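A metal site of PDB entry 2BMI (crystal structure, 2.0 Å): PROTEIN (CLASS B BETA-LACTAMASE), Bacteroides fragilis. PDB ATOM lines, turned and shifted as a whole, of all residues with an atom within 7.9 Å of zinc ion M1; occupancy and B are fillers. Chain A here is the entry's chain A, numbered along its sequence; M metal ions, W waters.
Zinc ion M1 is bound by water W1 (1.8 Å), NE2 of His 145 (2.1 Å), ND1 of His 84 (2.1 Å) and NE2 of His 82 (2.1 Å).
Asp 86 touches zinc ion M1 (OD1 to ZN, 3.9 Å). Of the 20 residues printed, 4 come within 4 Å of zinc ion M1.
OD1 of Asn 149 is in hydrogen-bond range of N of His 145 (3.0 Å). A ring nitrogen (NE2) of His 84 is in hydrogen-bond range of the side-chain carboxylate (OD2) of Asp 179 (2.7 Å). A ring nitrogen (ND1) of His 82 is in hydrogen-bond range of the side-chain sulfur (SG) of Cys 87 (3.3 Å). The side-chain amide oxygen of Asn 81 lies within hydrogen-bond range of a ring nitrogen (ND1) of His 82 (2.8 Å).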
ATOM      1  N   ASP A  52      -9.036   3.246  -8.971  1.00  0.00           N
ATOM      2  CA  ASP A  52      -9.496   3.280  -7.572  1.00  0.00           C
ATOM      3  C   ASP A  52      -8.777   4.379  -6.795  1.00  0.00           C
ATOM      4  O   ASP A  52      -7.567   4.612  -6.977  1.00  0.00           O
ATOM      5  CB  ASP A  52      -9.236   1.952  -6.838  1.00  0.00           C
ATOM      6  CG  ASP A  52     -10.345   0.921  -7.046  1.00  0.00           C
ATOM      7  OD1 ASP A  52     -11.075   1.008  -8.064  1.00  0.00           O
ATOM      8  OD2 ASP A  52     -10.464  -0.001  -6.194  1.00  0.00           O
ATOM      9  N   ASN A  81     -13.296   0.570  -9.379  1.00  0.00           N
ATOM     10  CA  ASN A  81     -13.731  -0.806  -9.517  1.00  0.00           C
ATOM     11  C   ASN A  81     -15.224  -0.926  -9.302  1.00  0.00           C
ATOM     12  O   ASN A  81     -15.917  -1.698  -9.961  1.00  0.00           O
ATOM     13  CB  ASN A  81     -13.021  -1.724  -8.535  1.00  0.00           C
ATOM     14  CG  ASN A  81     -13.318  -3.182  -8.793  1.00  0.00           C
ATOM     15  OD1 ASN A  81     -14.102  -3.794  -8.069  1.00  0.00           O
ATOM     16  ND2 ASN A  81     -12.719  -3.735  -9.838  1.00  0.00           N
ATOM     17  N   HIS A  82     -15.713  -0.208  -8.300  1.00  0.00           N
ATOM     18  CA  HIS A  82     -17.135  -0.176  -8.023  1.00  0.00           C
ATOM     19  C   HIS A  82     -17.489   1.038  -7.197  1.00  0.00           C
ATOM     20  O   HIS A  82     -16.669   1.949  -7.066  1.00  0.00           O
ATOM     21  CB  HIS A  82     -17.657  -1.504  -7.406  1.00  0.00           C
ATOM     22  CG  HIS A  82     -16.932  -1.943  -6.174  1.00  0.00           C
ATOM     23  ND1 HIS A  82     -15.662  -2.464  -6.186  1.00  0.00           N
ATOM     24  CD2 HIS A  82     -17.337  -1.935  -4.883  1.00  0.00           C
ATOM     25  CE1 HIS A  82     -15.346  -2.749  -4.931  1.00  0.00           C
ATOM     26  NE2 HIS A  82     -16.328  -2.438  -4.106  1.00  0.00           N
ATOM     27  N   TRP A  83     -18.701   1.080  -6.671  1.00  0.00           N
ATOM     28  CA  TRP A  83     -19.144   2.261  -5.920  1.00  0.00           C
ATOM     29  C   TRP A  83     -18.679   2.428  -4.477  1.00  0.00           C
ATOM     30  O   TRP A  83     -18.898   3.476  -3.912  1.00  0.00           O
ATOM     31  CB  TRP A  83     -20.688   2.420  -5.993  1.00  0.00           C
ATOM     32  CG  TRP A  83     -21.450   1.391  -5.230  1.00  0.00           C
ATOM     33  CD1 TRP A  83     -21.815   0.152  -5.661  1.00  0.00           C
ATOM     34  CD2 TRP A  83     -21.896   1.483  -3.863  1.00  0.00           C
ATOM     35  NE1 TRP A  83     -22.462  -0.532  -4.660  1.00  0.00           N
ATOM     36  CE2 TRP A  83     -22.531   0.268  -3.550  1.00  0.00           C
ATOM     37  CE3 TRP A  83     -21.835   2.493  -2.877  1.00  0.00           C
ATOM     38  CZ2 TRP A  83     -23.080   0.020  -2.282  1.00  0.00           C
ATOM     39  CZ3 TRP A  83     -22.376   2.243  -1.638  1.00  0.00           C
ATOM     40  CH2 TRP A  83     -23.002   1.025  -1.353  1.00  0.00           C
ATOM     41  N   HIS A  84     -18.032   1.426  -3.895  1.00  0.00           N
ATOM     42  CA  HIS A  84     -17.578   1.548  -2.504  1.00  0.00           C
ATOM     43  C   HIS A  84     -16.515   2.629  -2.261  1.00  0.00           C
ATOM     44  O   HIS A  84     -15.842   3.080  -3.195  1.00  0.00           O
ATOM     45  CB  HIS A  84     -17.131   0.206  -1.943  1.00  0.00           C
ATOM     46  CG  HIS A  84     -18.259  -0.726  -1.652  1.00  0.00           C
ATOM     47  ND1 HIS A  84     -18.085  -2.093  -1.547  1.00  0.00           N
ATOM     48  CD2 HIS A  84     -19.570  -0.435  -1.488  1.00  0.00           C
ATOM     49  CE1 HIS A  84     -19.278  -2.594  -1.329  1.00  0.00           C
ATOM     50  NE2 HIS A  84     -20.216  -1.642  -1.283  1.00  0.00           N
ATOM     51  N   GLY A  85     -16.364   3.017  -1.002  1.00  0.00           N
ATOM     52  CA  GLY A  85     -15.421   4.059  -0.656  1.00  0.00           C
ATOM     53  C   GLY A  85     -13.976   3.790  -1.002  1.00  0.00           C
ATOM     54  O   GLY A  85     -13.178   4.736  -1.204  1.00  0.00           O
ATOM     55  N   ASP A  86     -13.606   2.518  -0.993  1.00  0.00           N
ATOM     56  CA  ASP A  86     -12.245   2.133  -1.333  1.00  0.00           C
ATOM     57  C   ASP A  86     -11.982   2.174  -2.838  1.00  0.00           C
ATOM     58  O   ASP A  86     -10.883   1.808  -3.289  1.00  0.00           O
ATOM     59  CB  ASP A  86     -11.835   0.784  -0.710  1.00  0.00           C
ATOM     60  CG  ASP A  86     -12.842  -0.310  -0.925  1.00  0.00           C
ATOM     61  OD1 ASP A  86     -14.036  -0.086  -0.710  1.00  0.00           O
ATOM     62  OD2 ASP A  86     -12.401  -1.448  -1.250  1.00  0.00           O
ATOM     63  N   CYS A  87     -12.980   2.671  -3.580  1.00  0.00           N
ATOM     64  CA  CYS A  87     -12.908   2.823  -5.045  1.00  0.00           C
ATOM     65  C   CYS A  87     -13.132   4.288  -5.444  1.00  0.00           C
ATOM     66  O   CYS A  87     -12.414   4.811  -6.307  1.00  0.00           O
ATOM     67  CB  CYS A  87     -13.963   1.949  -5.751  1.00  0.00           C
ATOM     68  SG  CYS A  87     -13.862   0.214  -5.336  1.00  0.00           S
ATOM     69  N   HIS A 145     -18.347  -9.333  -5.658  1.00  0.00           N
ATOM     70  CA  HIS A 145     -18.213  -8.641  -4.375  1.00  0.00           C
ATOM     71  C   HIS A 145     -19.246  -7.491  -4.289  1.00  0.00           C
ATOM     72  O   HIS A 145     -19.693  -7.133  -3.194  1.00  0.00           O
ATOM     73  CB  HIS A 145     -16.803  -8.099  -4.239  1.00  0.00           C
ATOM     74  CG  HIS A 145     -16.683  -7.013  -3.231  1.00  0.00           C
ATOM     75  ND1 HIS A 145     -16.481  -7.247  -1.887  1.00  0.00           N
ATOM     76  CD2 HIS A 145     -16.718  -5.659  -3.377  1.00  0.00           C
ATOM     77  CE1 HIS A 145     -16.407  -6.062  -1.266  1.00  0.00           C
ATOM     78  NE2 HIS A 145     -16.554  -5.060  -2.130  1.00  0.00           N
ATOM     79  N   ALA A 146     -19.506  -6.847  -5.430  1.00  0.00           N
ATOM     80  CA  ALA A 146     -20.510  -5.786  -5.558  1.00  0.00           C
ATOM     81  C   ALA A 146     -21.192  -6.100  -6.887  1.00  0.00           C
ATOM     82  O   ALA A 146     -20.603  -6.727  -7.762  1.00  0.00           O
ATOM     83  CB  ALA A 146     -19.875  -4.423  -5.601  1.00  0.00           C
ATOM     84  N   ASP A 148     -21.891  -4.203  -9.385  1.00  0.00           N
ATOM     85  CA  ASP A 148     -21.305  -3.420 -10.463  1.00  0.00           C
ATOM     86  C   ASP A 148     -19.816  -3.591 -10.668  1.00  0.00           C
ATOM     87  O   ASP A 148     -19.232  -2.917 -11.519  1.00  0.00           O
ATOM     88  CB  ASP A 148     -21.603  -1.927 -10.217  1.00  0.00           C
ATOM     89  CG  ASP A 148     -20.967  -1.388  -8.920  1.00  0.00           C
ATOM     90  OD1 ASP A 148     -20.877  -2.128  -7.916  1.00  0.00           O
ATOM     91  OD2 ASP A 148     -20.564  -0.196  -8.892  1.00  0.00           O
ATOM     92  N   ASN A 149     -19.185  -4.508  -9.918  1.00  0.00           N
ATOM     93  CA  ASN A 149     -17.752  -4.655 -10.047  1.00  0.00           C
ATOM     94  C   ASN A 149     -17.248  -5.048 -11.436  1.00  0.00           C
ATOM     95  O   ASN A 149     -17.895  -5.796 -12.187  1.00  0.00           O
ATOM     96  CB  ASN A 149     -17.152  -5.536  -8.912  1.00  0.00           C
ATOM     97  CG  ASN A 149     -17.701  -6.955  -8.892  1.00  0.00           C
ATOM     98  OD1 ASN A 149     -17.404  -7.710  -7.982  1.00  0.00           O
ATOM     99  ND2 ASN A 149     -18.486  -7.324  -9.881  1.00  0.00           N
ATOM    100  N   GLY A 163      -9.604  -6.158  -8.675  1.00  0.00           N
ATOM    101  CA  GLY A 163     -10.383  -5.462  -7.674  1.00  0.00           C
ATOM    102  C   GLY A 163     -10.912  -6.369  -6.568  1.00  0.00           C
ATOM    103  O   GLY A 163     -10.485  -7.510  -6.406  1.00  0.00           O
ATOM    104  N   CYS A 164     -11.888  -5.836  -5.842  1.00  0.00           N
ATOM    105  CA  CYS A 164     -12.489  -6.504  -4.714  1.00  0.00           C
ATOM    106  C   CYS A 164     -13.193  -7.821  -4.957  1.00  0.00           C
ATOM    107  O   CYS A 164     -13.538  -8.496  -3.993  1.00  0.00           O
ATOM    108  CB  CYS A 164     -13.370  -5.509  -3.975  1.00  0.00           C
ATOM    109  SG  CYS A 164     -12.431  -4.062  -3.400  1.00  0.00           S
ATOM    110  N   MET A 165     -13.450  -8.197  -6.218  1.00  0.00           N
ATOM    111  CA  MET A 165     -14.087  -9.480  -6.485  1.00  0.00           C
ATOM    112  C   MET A 165     -13.086 -10.605  -6.290  1.00  0.00           C
ATOM    113  O   MET A 165     -13.440 -11.792  -6.304  1.00  0.00           O
ATOM    114  CB  MET A 165     -14.618  -9.532  -7.925  1.00  0.00           C
ATOM    115  CG  MET A 165     -13.510  -9.575  -8.995  1.00  0.00           C
ATOM    116  SD  MET A 165     -14.218 -10.066 -10.569  1.00  0.00           S
ATOM    117  CE  MET A 165     -15.222  -8.643 -11.007  1.00  0.00           C
ATOM    118  N   ASN A 176     -16.604  -8.316   3.378  1.00  0.00           N
ATOM    119  CA  ASN A 176     -17.834  -7.529   3.298  1.00  0.00           C
ATOM    120  C   ASN A 176     -18.733  -7.929   2.173  1.00  0.00           C
ATOM    121  O   ASN A 176     -18.456  -7.580   1.015  1.00  0.00           O
ATOM    122  CB  ASN A 176     -17.507  -6.038   3.154  1.00  0.00           C
ATOM    123  CG  ASN A 176     -18.773  -5.167   3.025  1.00  0.00           C
ATOM    124  OD1 ASN A 176     -19.815  -5.491   3.599  1.00  0.00           O
ATOM    125  ND2 ASN A 176     -18.665  -4.063   2.292  1.00  0.00           N
ATOM    126  N   SER A 178     -22.170  -7.103   2.115  1.00  0.00           N
ATOM    127  CA  SER A 178     -23.417  -6.344   2.178  1.00  0.00           C
ATOM    128  C   SER A 178     -23.991  -5.968   0.807  1.00  0.00           C
ATOM    129  O   SER A 178     -25.194  -5.780   0.666  1.00  0.00           O
ATOM    130  CB  SER A 178     -23.241  -5.080   3.001  1.00  0.00           C
ATOM    131  OG  SER A 178     -22.302  -4.226   2.377  1.00  0.00           O
ATOM    132  N   ASP A 179     -23.123  -5.811  -0.192  1.00  0.00           N
ATOM    133  CA  ASP A 179     -23.598  -5.466  -1.531  1.00  0.00           C
ATOM    134  C   ASP A 179     -23.175  -6.539  -2.505  1.00  0.00           C
ATOM    135  O   ASP A 179     -23.095  -6.299  -3.702  1.00  0.00           O
ATOM    136  CB  ASP A 179     -23.012  -4.113  -1.943  1.00  0.00           C
ATOM    137  CG  ASP A 179     -23.407  -3.011  -1.005  1.00  0.00           C
ATOM    138  OD1 ASP A 179     -24.603  -2.668  -1.009  1.00  0.00           O
ATOM    139  OD2 ASP A 179     -22.563  -2.528  -0.227  1.00  0.00           O
ATOM    140  N   GLY A 205      -8.591  -6.259  -4.466  1.00  0.00           N
ATOM    141  CA  GLY A 205      -8.980  -4.989  -3.863  1.00  0.00           C
ATOM    142  C   GLY A 205      -8.294  -4.715  -2.531  1.00  0.00           C
ATOM    143  O   GLY A 205      -8.098  -3.557  -2.175  1.00  0.00           O
ATOM    144  N   HIS A 206      -7.967  -5.787  -1.796  1.00  0.00           N
ATOM    145  CA  HIS A 206      -7.282  -5.708  -0.501  1.00  0.00           C
ATOM    146  C   HIS A 206      -6.283  -6.875  -0.429  1.00  0.00           C
ATOM    147  O   HIS A 206      -6.584  -7.990  -0.871  1.00  0.00           O
ATOM    148  CB  HIS A 206      -8.289  -5.840   0.643  1.00  0.00           C
ATOM    149  CG  HIS A 206      -9.461  -4.902   0.527  1.00  0.00           C
ATOM    150  ND1 HIS A 206      -9.440  -3.597   0.966  1.00  0.00           N
ATOM    151  CD2 HIS A 206     -10.663  -5.071  -0.068  1.00  0.00           C
ATOM    152  CE1 HIS A 206     -10.602  -3.023   0.618  1.00  0.00           C
ATOM    153  NE2 HIS A 206     -11.389  -3.869  -0.010  1.00  0.00           N
HETATM  154 ZN    ZN M   1     -16.295  -3.018  -2.054  1.00  0.00          ZN
HETATM  155 ZN    ZN M   2     -13.028  -3.508  -1.130  1.00  0.00          ZN
HETATM  156  O   HOH W   1     -14.808  -2.902  -1.088  1.00  0.00           O
